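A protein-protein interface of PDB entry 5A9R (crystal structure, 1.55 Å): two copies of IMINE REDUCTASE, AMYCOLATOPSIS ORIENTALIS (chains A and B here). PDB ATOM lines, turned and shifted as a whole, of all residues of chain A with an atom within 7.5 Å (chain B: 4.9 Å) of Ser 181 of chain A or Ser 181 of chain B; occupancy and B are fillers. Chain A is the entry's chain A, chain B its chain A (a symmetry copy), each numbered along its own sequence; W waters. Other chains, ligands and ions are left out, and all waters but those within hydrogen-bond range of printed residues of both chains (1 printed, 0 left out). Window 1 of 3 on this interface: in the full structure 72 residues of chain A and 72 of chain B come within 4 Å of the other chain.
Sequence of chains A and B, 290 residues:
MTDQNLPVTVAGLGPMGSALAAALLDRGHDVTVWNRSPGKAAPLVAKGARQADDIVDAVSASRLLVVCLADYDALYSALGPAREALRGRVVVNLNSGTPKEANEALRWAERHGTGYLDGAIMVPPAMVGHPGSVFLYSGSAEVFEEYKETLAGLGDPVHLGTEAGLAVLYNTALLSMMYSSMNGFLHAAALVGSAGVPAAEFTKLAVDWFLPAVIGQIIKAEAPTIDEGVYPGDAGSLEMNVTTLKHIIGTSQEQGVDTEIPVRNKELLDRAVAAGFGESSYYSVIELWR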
ATOM      1  N   LEU A 174       8.451   3.291 -23.917  1.00  0.00           N
ATOM      2  CA  LEU A 174       9.012   3.400 -25.274  1.00  0.00           C
ATOM      3  C   LEU A 174       9.238   4.845 -25.678  1.00  0.00           C
ATOM      4  O   LEU A 174      10.316   5.184 -26.260  1.00  0.00           O
ATOM      5  CB  LEU A 174       8.122   2.642 -26.280  1.00  0.00           C
ATOM      6  CG  LEU A 174       8.101   1.146 -26.098  1.00  0.00           C
ATOM      7  CD1 LEU A 174       7.008   0.549 -26.943  1.00  0.00           C
ATOM      8  CD2 LEU A 174       9.478   0.525 -26.389  1.00  0.00           C
ATOM      9  N   LEU A 175       8.314   5.714 -25.329  1.00  0.00           N
ATOM     10  CA  LEU A 175       8.499   7.164 -25.643  1.00  0.00           C
ATOM     11  C   LEU A 175       9.652   7.757 -24.835  1.00  0.00           C
ATOM     12  O   LEU A 175      10.415   8.561 -25.377  1.00  0.00           O
ATOM     13  CB  LEU A 175       7.228   7.940 -25.397  1.00  0.00           C
ATOM     14  CG  LEU A 175       6.121   7.613 -26.369  1.00  0.00           C
ATOM     15  CD1 LEU A 175       4.827   8.278 -25.872  1.00  0.00           C
ATOM     16  CD2 LEU A 175       6.408   8.055 -27.804  1.00  0.00           C
ATOM     17  N   SER A 176       9.842   7.337 -23.604  1.00  0.00           N
ATOM     18  CA  SER A 176      10.973   7.826 -22.787  1.00  0.00           C
ATOM     19  C   SER A 176      12.273   7.470 -23.445  1.00  0.00           C
ATOM     20  O   SER A 176      13.201   8.245 -23.568  1.00  0.00           O
ATOM     21  CB  SER A 176      10.843   7.274 -21.398  1.00  0.00           C
ATOM     22  OG  SER A 176      11.803   7.891 -20.539  1.00  0.00           O
ATOM     23  N   MET A 177      12.323   6.198 -23.882  1.00  0.00           N
ATOM     24  CA  MET A 177      13.514   5.709 -24.614  1.00  0.00           C
ATOM     25  C   MET A 177      13.752   6.487 -25.887  1.00  0.00           C
ATOM     26  O   MET A 177      14.909   6.842 -26.245  1.00  0.00           O
ATOM     27  CB  MET A 177      13.362   4.202 -24.923  1.00  0.00           C
ATOM     28  CG  MET A 177      14.567   3.648 -25.620  1.00  0.00           C
ATOM     29  SD  MET A 177      14.325   1.843 -25.916  1.00  0.00           S
ATOM     30  CE  MET A 177      13.214   1.793 -27.188  1.00  0.00           C
ATOM     31  N   MET A 178      12.683   6.784 -26.648  1.00  0.00           N
ATOM     32  CA  MET A 178      12.764   7.545 -27.872  1.00  0.00           C
ATOM     33  C   MET A 178      13.428   8.926 -27.642  1.00  0.00           C
ATOM     34  O   MET A 178      14.288   9.344 -28.365  1.00  0.00           O
ATOM     35  CB  MET A 178      11.322   7.686 -28.498  1.00  0.00           C
ATOM     36  CG  MET A 178      11.306   8.503 -29.757  1.00  0.00           C
ATOM     37  SD  MET A 178       9.591   8.946 -30.206  1.00  0.00           S
ATOM     38  CE  MET A 178       9.271  10.156 -28.890  1.00  0.00           C
ATOM     39  N   TYR A 179      12.920   9.668 -26.631  1.00  0.00           N
ATOM     40  CA  TYR A 179      13.457  11.036 -26.441  1.00  0.00           C
ATOM     41  C   TYR A 179      14.950  10.994 -26.084  1.00  0.00           C
ATOM     42  O   TYR A 179      15.723  11.782 -26.669  1.00  0.00           O
ATOM     43  CB  TYR A 179      12.714  11.776 -25.365  1.00  0.00           C
ATOM     44  CG  TYR A 179      11.330  12.278 -25.796  1.00  0.00           C
ATOM     45  CD1 TYR A 179      11.232  13.250 -26.766  1.00  0.00           C
ATOM     46  CD2 TYR A 179      10.171  11.728 -25.277  1.00  0.00           C
ATOM     47  CE1 TYR A 179       9.987  13.636 -27.279  1.00  0.00           C
ATOM     48  CE2 TYR A 179       8.937  12.120 -25.764  1.00  0.00           C
ATOM     49  CZ  TYR A 179       8.858  13.069 -26.722  1.00  0.00           C
ATOM     50  OH  TYR A 179       7.621  13.502 -27.245  1.00  0.00           O
ATOM     51  N   SER A 180      15.366  10.070 -25.218  1.00  0.00           N
ATOM     52  CA  SER A 180      16.754   9.950 -24.895  1.00  0.00           C
ATOM     53  C   SER A 180      17.622   9.581 -26.116  1.00  0.00           C
ATOM     54  O   SER A 180      18.707  10.141 -26.410  1.00  0.00           O
ATOM     55  CB  SER A 180      16.945   8.912 -23.829  1.00  0.00           C
ATOM     56  OG  SER A 180      16.657   9.415 -22.488  1.00  0.00           O
ATOM     57  N   SER A 181      17.106   8.630 -26.884  1.00  0.00           N
ATOM     58  CA  SER A 181      17.842   8.168 -28.109  1.00  0.00           C
ATOM     59  C   SER A 181      17.970   9.246 -29.141  1.00  0.00           C
ATOM     60  O   SER A 181      19.031   9.492 -29.734  1.00  0.00           O
ATOM     61  CB  SER A 181      17.159   6.938 -28.738  1.00  0.00           C
ATOM     62  OG  SER A 181      17.070   5.907 -27.831  1.00  0.00           O
ATOM     63  N   MET A 182      16.893  10.046 -29.370  1.00  0.00           N
ATOM     64  CA  MET A 182      16.887  11.126 -30.299  1.00  0.00           C
ATOM     65  C   MET A 182      17.856  12.226 -29.847  1.00  0.00           C
ATOM     66  O   MET A 182      18.583  12.796 -30.683  1.00  0.00           O
ATOM     67  CB  MET A 182      15.468  11.741 -30.518  1.00  0.00           C
ATOM     68  CG  MET A 182      14.715  10.741 -31.381  1.00  0.00           C
ATOM     69  SD  MET A 182      13.057  11.185 -31.825  1.00  0.00           S
ATOM     70  CE  MET A 182      12.506  12.550 -30.779  1.00  0.00           C
ATOM     71  N   ASN A 183      17.883  12.509 -28.529  1.00  0.00           N
ATOM     72  CA  ASN A 183      18.814  13.501 -28.061  1.00  0.00           C
ATOM     73  C   ASN A 183      20.260  13.055 -28.246  1.00  0.00           C
ATOM     74  O   ASN A 183      21.104  13.881 -28.636  1.00  0.00           O
ATOM     75  CB  ASN A 183      18.550  13.870 -26.620  1.00  0.00           C
ATOM     76  CG  ASN A 183      17.227  14.575 -26.427  1.00  0.00           C
ATOM     77  OD1 ASN A 183      16.743  14.617 -25.263  1.00  0.00           O
ATOM     78  ND2 ASN A 183      16.675  15.075 -27.419  1.00  0.00           N
ATOM     79  N   GLY A 184      20.506  11.766 -28.063  1.00  0.00           N
ATOM     80  CA  GLY A 184      21.836  11.215 -28.361  1.00  0.00           C
ATOM     81  C   GLY A 184      22.182  11.328 -29.816  1.00  0.00           C
ATOM     82  O   GLY A 184      23.293  11.796 -30.165  1.00  0.00           O
ATOM     83  N   PHE A 185      21.212  11.040 -30.704  1.00  0.00           N
ATOM     84  CA  PHE A 185      21.492  11.234 -32.100  1.00  0.00           C
ATOM     85  C   PHE A 185      21.806  12.659 -32.496  1.00  0.00           C
ATOM     86  O   PHE A 185      22.722  12.964 -33.281  1.00  0.00           O
ATOM     87  CB  PHE A 185      20.324  10.711 -32.970  1.00  0.00           C
ATOM     88  CG  PHE A 185      20.512  11.069 -34.382  1.00  0.00           C
ATOM     89  CD1 PHE A 185      21.354  10.286 -35.172  1.00  0.00           C
ATOM     90  CD2 PHE A 185      19.931  12.198 -34.919  1.00  0.00           C
ATOM     91  CE1 PHE A 185      21.614  10.697 -36.498  1.00  0.00           C
ATOM     92  CE2 PHE A 185      20.219  12.616 -36.235  1.00  0.00           C
ATOM     93  CZ  PHE A 185      21.017  11.824 -37.044  1.00  0.00           C
ATOM     94  N   LEU A 186      21.061  13.621 -31.891  1.00  0.00           N
ATOM     95  CA  LEU A 186      21.285  15.010 -32.169  1.00  0.00           C
ATOM     96  C   LEU A 186      22.647  15.534 -31.709  1.00  0.00           C
ATOM     97  O   LEU A 186      23.336  16.275 -32.422  1.00  0.00           O
ATOM     98  CB  LEU A 186      20.140  15.804 -31.590  1.00  0.00           C
ATOM     99  CG  LEU A 186      18.773  15.552 -32.264  1.00  0.00           C
ATOM    100  CD1 LEU A 186      17.698  16.286 -31.429  1.00  0.00           C
ATOM    101  CD2 LEU A 186      18.782  16.042 -33.674  1.00  0.00           C
ATOM    102  N   HIS A 187      23.139  15.023 -30.569  1.00  0.00           N
ATOM    103  CA  HIS A 187      24.497  15.381 -30.157  1.00  0.00           C
ATOM    104  C   HIS A 187      25.551  14.796 -31.105  1.00  0.00           C
ATOM    105  O   HIS A 187      26.490  15.467 -31.521  1.00  0.00           O
ATOM    106  CB  HIS A 187      24.748  14.935 -28.697  1.00  0.00           C
ATOM    107  CG  HIS A 187      26.034  15.397 -28.198  1.00  0.00           C
ATOM    108  ND1 HIS A 187      27.111  14.585 -28.017  1.00  0.00           N
ATOM    109  CD2 HIS A 187      26.462  16.668 -27.942  1.00  0.00           C
ATOM    110  CE1 HIS A 187      28.148  15.320 -27.661  1.00  0.00           C
ATOM    111  NE2 HIS A 187      27.795  16.580 -27.654  1.00  0.00           N
ATOM    112  N   PHE A 210      24.671   1.302 -36.967  1.00  0.00           N
ATOM    113  CA  PHE A 210      25.040   1.348 -35.540  1.00  0.00           C
ATOM    114  C   PHE A 210      23.846   1.092 -34.596  1.00  0.00           C
ATOM    115  O   PHE A 210      23.966   0.366 -33.600  1.00  0.00           O
ATOM    116  CB  PHE A 210      25.747   2.659 -35.235  1.00  0.00           C
ATOM    117  CG  PHE A 210      26.400   2.679 -33.893  1.00  0.00           C
ATOM    118  CD1 PHE A 210      27.647   2.129 -33.695  1.00  0.00           C
ATOM    119  CD2 PHE A 210      25.812   3.409 -32.857  1.00  0.00           C
ATOM    120  CE1 PHE A 210      28.300   2.241 -32.444  1.00  0.00           C
ATOM    121  CE2 PHE A 210      26.415   3.449 -31.597  1.00  0.00           C
ATOM    122  CZ  PHE A 210      27.650   2.873 -31.418  1.00  0.00           C
ATOM    123  N   LEU A 211      22.735   1.754 -34.906  1.00  0.00           N
ATOM    124  CA  LEU A 211      21.597   1.635 -34.025  1.00  0.00           C
ATOM    125  C   LEU A 211      21.149   0.219 -33.785  1.00  0.00           C
ATOM    126  O   LEU A 211      21.102  -0.224 -32.624  1.00  0.00           O
ATOM    127  CB  LEU A 211      20.493   2.556 -34.508  1.00  0.00           C
ATOM    128  CG  LEU A 211      19.214   2.633 -33.724  1.00  0.00           C
ATOM    129  CD1 LEU A 211      19.535   3.396 -32.462  1.00  0.00           C
ATOM    130  CD2 LEU A 211      18.200   3.402 -34.493  1.00  0.00           C
ATOM    131  N   ILE A 215      23.931  -0.723 -30.800  1.00  0.00           N
ATOM    132  CA  ILE A 215      23.080  -0.332 -29.648  1.00  0.00           C
ATOM    133  C   ILE A 215      22.055  -1.408 -29.322  1.00  0.00           C
ATOM    134  O   ILE A 215      21.967  -1.872 -28.176  1.00  0.00           O
ATOM    135  CB  ILE A 215      22.394   1.017 -29.834  1.00  0.00           C
ATOM    136  CG1 ILE A 215      23.470   2.155 -29.968  1.00  0.00           C
ATOM    137  CG2 ILE A 215      21.342   1.308 -28.790  1.00  0.00           C
ATOM    138  CD1 ILE A 215      22.931   3.466 -30.426  1.00  0.00           C
ATOM    139  N   GLY A 216      21.334  -1.862 -30.327  1.00  0.00           N
ATOM    140  CA  GLY A 216      20.342  -2.856 -30.083  1.00  0.00           C
ATOM    141  C   GLY A 216      20.867  -4.181 -29.611  1.00  0.00           C
ATOM    142  O   GLY A 216      20.364  -4.821 -28.689  1.00  0.00           O
ATOM    143  N   ILE A 219      21.968  -3.938 -25.939  1.00  0.00           N
ATOM    144  CA  ILE A 219      20.852  -3.993 -25.056  1.00  0.00           C
ATOM    145  C   ILE A 219      20.343  -5.458 -24.933  1.00  0.00           C
ATOM    146  O   ILE A 219      20.078  -5.869 -23.821  1.00  0.00           O
ATOM    147  CB  ILE A 219      19.709  -3.079 -25.557  1.00  0.00           C
ATOM    148  CG1 ILE A 219      20.090  -1.603 -25.454  1.00  0.00           C
ATOM    149  CG2 ILE A 219      18.413  -3.347 -24.731  1.00  0.00           C
ATOM    150  CD1 ILE A 219      19.182  -0.619 -26.208  1.00  0.00           C
ATOM    151  N   ASN A 265      25.079  12.606 -19.021  1.00  0.00           N
ATOM    152  CA  ASN A 265      25.373  11.186 -18.966  1.00  0.00           C
ATOM    153  C   ASN A 265      26.438  10.791 -17.952  1.00  0.00           C
ATOM    154  O   ASN A 265      26.321   9.803 -17.187  1.00  0.00           O
ATOM    155  CB  ASN A 265      25.681  10.665 -20.410  1.00  0.00           C
ATOM    156  CG  ASN A 265      24.430  10.584 -21.312  1.00  0.00           C
ATOM    157  OD1 ASN A 265      23.298  10.450 -20.855  1.00  0.00           O
ATOM    158  ND2 ASN A 265      24.609  10.721 -22.601  1.00  0.00           N
ATOM    159  N   TYR A 282      27.895  -1.271 -16.167  1.00  0.00           N
ATOM    160  CA  TYR A 282      27.164  -0.050 -16.546  1.00  0.00           C
ATOM    161  C   TYR A 282      25.701  -0.161 -16.186  1.00  0.00           C
ATOM    162  O   TYR A 282      25.112   0.706 -15.586  1.00  0.00           O
ATOM    163  CB  TYR A 282      27.317   0.162 -18.099  1.00  0.00           C
ATOM    164  CG  TYR A 282      26.731   1.463 -18.562  1.00  0.00           C
ATOM    165  CD1 TYR A 282      25.322   1.640 -18.693  1.00  0.00           C
ATOM    166  CD2 TYR A 282      27.516   2.572 -18.748  1.00  0.00           C
ATOM    167  CE1 TYR A 282      24.812   2.857 -19.077  1.00  0.00           C
ATOM    168  CE2 TYR A 282      26.982   3.786 -19.090  1.00  0.00           C
ATOM    169  CZ  TYR A 282      25.576   3.913 -19.306  1.00  0.00           C
ATOM    170  OH  TYR A 282      25.069   5.166 -19.583  1.00  0.00           O
ATOM    171  N   MET B 177      25.853   8.888 -28.770  1.00  0.00           N
ATOM    172  CA  MET B 177      24.485   8.404 -29.065  1.00  0.00           C
ATOM    173  C   MET B 177      24.158   7.140 -28.304  1.00  0.00           C
ATOM    174  O   MET B 177      23.033   6.961 -27.761  1.00  0.00           O
ATOM    175  CB  MET B 177      24.320   8.176 -30.585  1.00  0.00           C
ATOM    176  CG  MET B 177      22.934   7.734 -30.940  1.00  0.00           C
ATOM    177  SD  MET B 177      22.808   7.523 -32.768  1.00  0.00           S
ATOM    178  CE  MET B 177      23.649   6.087 -33.063  1.00  0.00           C
ATOM    179  N   MET B 178      25.108   6.190 -28.232  1.00  0.00           N
ATOM    180  CA  MET B 178      24.940   4.949 -27.514  1.00  0.00           C
ATOM    181  C   MET B 178      24.572   5.194 -26.028  1.00  0.00           C
ATOM    182  O   MET B 178      23.680   4.602 -25.490  1.00  0.00           O
ATOM    183  CB  MET B 178      26.249   4.080 -27.657  1.00  0.00           C
ATOM    184  CG  MET B 178      26.177   2.783 -26.903  1.00  0.00           C
ATOM    185  SD  MET B 178      27.835   2.021 -26.791  1.00  0.00           S
ATOM    186  CE  MET B 178      28.586   3.178 -25.610  1.00  0.00           C
ATOM    187  N   TYR B 179      25.371   6.052 -25.353  1.00  0.00           N
ATOM    188  CA  TYR B 179      25.118   6.238 -23.905  1.00  0.00           C
ATOM    189  C   TYR B 179      23.728   6.845 -23.666  1.00  0.00           C
ATOM    190  O   TYR B 179      23.007   6.348 -22.774  1.00  0.00           O
ATOM    191  CB  TYR B 179      26.156   7.118 -23.271  1.00  0.00           C
ATOM    192  CG  TYR B 179      27.505   6.426 -23.042  1.00  0.00           C
ATOM    193  CD1 TYR B 179      27.591   5.390 -22.139  1.00  0.00           C
ATOM    194  CD2 TYR B 179      28.628   6.777 -23.770  1.00  0.00           C
ATOM    195  CE1 TYR B 179      28.771   4.648 -22.001  1.00  0.00           C
ATOM    196  CE2 TYR B 179      29.803   6.062 -23.624  1.00  0.00           C
ATOM    197  CZ  TYR B 179      29.869   5.043 -22.740  1.00  0.00           C
ATOM    198  OH  TYR B 179      31.047   4.289 -22.555  1.00  0.00           O
ATOM    199  N   SER B 180      23.322   7.829 -24.468  1.00  0.00           N
ATOM    200  CA  SER B 180      22.015   8.390 -24.326  1.00  0.00           C
ATOM    201  C   SER B 180      20.893   7.363 -24.578  1.00  0.00           C
ATOM    202  O   SER B 180      19.883   7.220 -23.844  1.00  0.00           O
ATOM    203  CB  SER B 180      21.844   9.542 -25.273  1.00  0.00           C
ATOM    204  OG  SER B 180      22.449  10.777 -24.780  1.00  0.00           O
ATOM    205  N   SER B 181      21.094   6.584 -25.633  1.00  0.00           N
ATOM    206  CA  SER B 181      20.082   5.537 -26.001  1.00  0.00           C
ATOM    207  C   SER B 181      19.956   4.471 -24.956  1.00  0.00           C
ATOM    208  O   SER B 181      18.864   4.051 -24.546  1.00  0.00           O
ATOM    209  CB  SER B 181      20.423   4.885 -27.356  1.00  0.00           C
ATOM    210  OG  SER B 181      20.496   5.831 -28.352  1.00  0.00           O
ATOM    211  N   MET B 182      21.095   4.009 -24.370  1.00  0.00           N
ATOM    212  CA  MET B 182      21.118   3.021 -23.344  1.00  0.00           C
ATOM    213  C   MET B 182      20.446   3.555 -22.072  1.00  0.00           C
ATOM    214  O   MET B 182      19.689   2.818 -21.412  1.00  0.00           O
ATOM    215  CB  MET B 182      22.558   2.523 -23.002  1.00  0.00           C
ATOM    216  CG  MET B 182      22.963   1.614 -24.151  1.00  0.00           C
ATOM    217  SD  MET B 182      24.566   0.866 -24.028  1.00  0.00           S
ATOM    218  CE  MET B 182      25.520   1.709 -22.746  1.00  0.00           C
ATOM    219  N   ASN B 183      20.704   4.836 -21.741  1.00  0.00           N
ATOM    220  CA  ASN B 183      20.055   5.388 -20.581  1.00  0.00           C
ATOM    221  C   ASN B 183      18.544   5.481 -20.767  1.00  0.00           C
ATOM    222  O   ASN B 183      17.797   5.186 -19.819  1.00  0.00           O
ATOM    223  CB  ASN B 183      20.631   6.734 -20.213  1.00  0.00           C
ATOM    224  CG  ASN B 183      22.068   6.652 -19.750  1.00  0.00           C
ATOM    225  OD1 ASN B 183      22.752   7.711 -19.752  1.00  0.00           O
ATOM    226  ND2 ASN B 183      22.510   5.549 -19.393  1.00  0.00           N
ATOM    227  N   GLY B 184      18.120   5.791 -21.985  1.00  0.00           N
ATOM    228  CA  GLY B 184      16.684   5.761 -22.299  1.00  0.00           C
ATOM    229  C   GLY B 184      16.108   4.381 -22.179  1.00  0.00           C
ATOM    230  O   GLY B 184      15.048   4.196 -21.533  1.00  0.00           O
ATOM    231  N   PHE B 185      16.839   3.363 -22.669  1.00  0.00           N
ATOM    232  CA  PHE B 185      16.351   2.025 -22.479  1.00  0.00           C
ATOM    233  C   PHE B 185      16.218   1.592 -21.036  1.00  0.00           C
ATOM    234  O   PHE B 185      15.241   0.956 -20.601  1.00  0.00           O
ATOM    235  CB  PHE B 185      17.238   1.007 -23.235  1.00  0.00           C
ATOM    236  CG  PHE B 185      16.864  -0.374 -22.901  1.00  0.00           C
ATOM    237  CD1 PHE B 185      15.774  -0.954 -23.549  1.00  0.00           C
ATOM    238  CD2 PHE B 185      17.522  -1.077 -21.915  1.00  0.00           C
ATOM    239  CE1 PHE B 185      15.354  -2.242 -23.147  1.00  0.00           C
ATOM    240  CE2 PHE B 185      17.079  -2.350 -21.501  1.00  0.00           C
ATOM    241  CZ  PHE B 185      16.026  -2.957 -22.166  1.00  0.00           C
ATOM    242  N   LEU B 211      13.033   0.119 -31.680  1.00  0.00           N
ATOM    243  CA  LEU B 211      14.274   0.800 -31.969  1.00  0.00           C
ATOM    244  C   LEU B 211      14.510   1.056 -33.432  1.00  0.00           C
ATOM    245  O   LEU B 211      14.689   2.219 -33.833  1.00  0.00           O
ATOM    246  CB  LEU B 211      15.413   0.076 -31.278  1.00  0.00           C
ATOM    247  CG  LEU B 211      16.807   0.624 -31.403  1.00  0.00           C
ATOM    248  CD1 LEU B 211      16.851   1.867 -30.549  1.00  0.00           C
ATOM    249  CD2 LEU B 211      17.782  -0.357 -30.857  1.00  0.00           C
ATOM    250  N   ILE B 215      12.189   4.527 -33.750  1.00  0.00           N
ATOM    251  CA  ILE B 215      13.287   5.488 -33.475  1.00  0.00           C
ATOM    252  C   ILE B 215      14.156   5.708 -34.705  1.00  0.00           C
ATOM    253  O   ILE B 215      14.368   6.851 -35.135  1.00  0.00           O
ATOM    254  CB  ILE B 215      14.147   5.097 -32.279  1.00  0.00           C
ATOM    255  CG1 ILE B 215      13.274   5.072 -30.973  1.00  0.00           C
ATOM    256  CG2 ILE B 215      15.403   5.926 -32.143  1.00  0.00           C
ATOM    257  CD1 ILE B 215      13.937   4.442 -29.797  1.00  0.00           C
HETATM  258  O   HOH W   1      25.537   7.739 -19.009  1.00  0.00           O
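Water W1 lies within hydrogen-bond range of OH of Tyr 282 of chain A, O of Asn 265 of chain A and OD1 of Asn 183 of chain B.
Among the printed residues, merely in contact across the chains: Met 177 of chain A with Gly 184 of chain B, Met 177 of chain A with Phe 185 of chain B, Met 177 of chain A with Ile 215 of chain B, Met 178 of chain A with Ile 215 of chain B, Ser 180 of chain A with Ser 180 of chain B, Ser 180 of chain A with Gly 184 of chain B, Ser 181 of chain A with Ile 215 of chain B, Gly 184 of chain A with Met 177 of chain B, Gly 184 of chain A with Ser 180 of chain B, Phe 185 of chain A with Met 177 of chain B, Phe 210 of chain A with Met 177 of chain B, Phe 210 of chain A with Met 178 of chain B, Leu 211 of chain A with Leu 211 of chain B, Ile 215 of chain A with Met 177 of chain B, Ile 215 of chain A with Met 178 of chain B, Ile 215 of chain A with Ser 181 of chain B, Gly 216 of chain A with Leu 211 of chain B, Ile 219 of chain A with Phe 185 of chain B, Asn 265 of chain A with Tyr 179 of chain B, Tyr 282 of chain A with Tyr 179 of chain B and Tyr 282 of chain A with Met 182 of chain B.
Met 177 of chain A touches Gly 184 of chain B, and with the chains exchanged Gly 184 of chain A touches Met 177 of chain B.
Met 178 of chain A touches Ile 215 of chain B, and with the chains exchanged Ile 215 of chain A touches Met 178 of chain B.
Ser 180 of chain A touches Gly 184 of chain B, and with the chains exchanged Gly 184 of chain A touches Ser 180 of chain B.
Ser 181 of chain A touches Ile 215 of chain B, and with the chains exchanged Ile 215 of chain A touches Ser 181 of chain B.
Positions printed for both chains: 177, 178, 179, 180, 181, 182, 183, 184, 185, 211 and 215.
Of the 25 pairs that touch across the chains among the printed residues, 15 have their exchanged pair printed and touching as well.
Ser 181 of chain B touches two residues of chain A.
Of the printed residues of chain B, Tyr 282 of chain A touches Tyr 179 (3.5 Å), Met 182 (3.9 Å) and Asn 183 (2.6 Å).
Printed residues of chain A within 4 Å of Ser 180 of chain B: Ser 180, Gly 184 and Asn 265.
Ser 176 of chain A touches none of the printed residues of chain B.
Leu 174 of chain A touches none of the printed residues of chain B.
Of the 21 printed residues of chain A, 13 touch a printed residue of chain B.
Hydrophobic or aromatic side chains of chain B within 4 Å of the printed part of chain A: Met 177, Met 178, Tyr 179, Met 182, Phe 185, Leu 211 and Ile 215.
The backbone carbonyl oxygen (O) of Met 177 of chain A lies within hydrogen-bond range of the side-chain hydroxyl (OG) of Ser 181 of chain A, at 2.8 Å.
The backbone carbonyl oxygen of Phe 210 of chain A is in hydrogen-bond range of the backbone NH of Ile 215 of chain A.
O of Leu 211 of chain A sits at hydrogen-bond distance from N of Gly 216 of chain A (2.8 Å).
O of Met 177 of chain B is in hydrogen-bond range of OG of Ser 181 of chain B (2.8 Å).
O of Tyr 179 of chain B lies close to OD1 of Asn 183 of chain B (3.3 Å).
OG of Ser 181 of chain B is in hydrogen-bond range of OG of Ser 181 of chain A, at 3.5 Å.
The side-chain amide nitrogen (ND2) of Asn 265 of chain A lies within hydrogen-bond range of the side-chain hydroxyl (OG) of Ser 180 of chain B (3.1 Å).
The side-chain amide oxygen (OD1) of Asn 265 of chain A sits close to the side-chain amide oxygen (OD1) of Asn 183 of chain B, 3.0 Å away.
OH of Tyr 282 of chain A sits at hydrogen-bond distance from ND2 of Asn 183 of chain B, 2.6 Å away.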
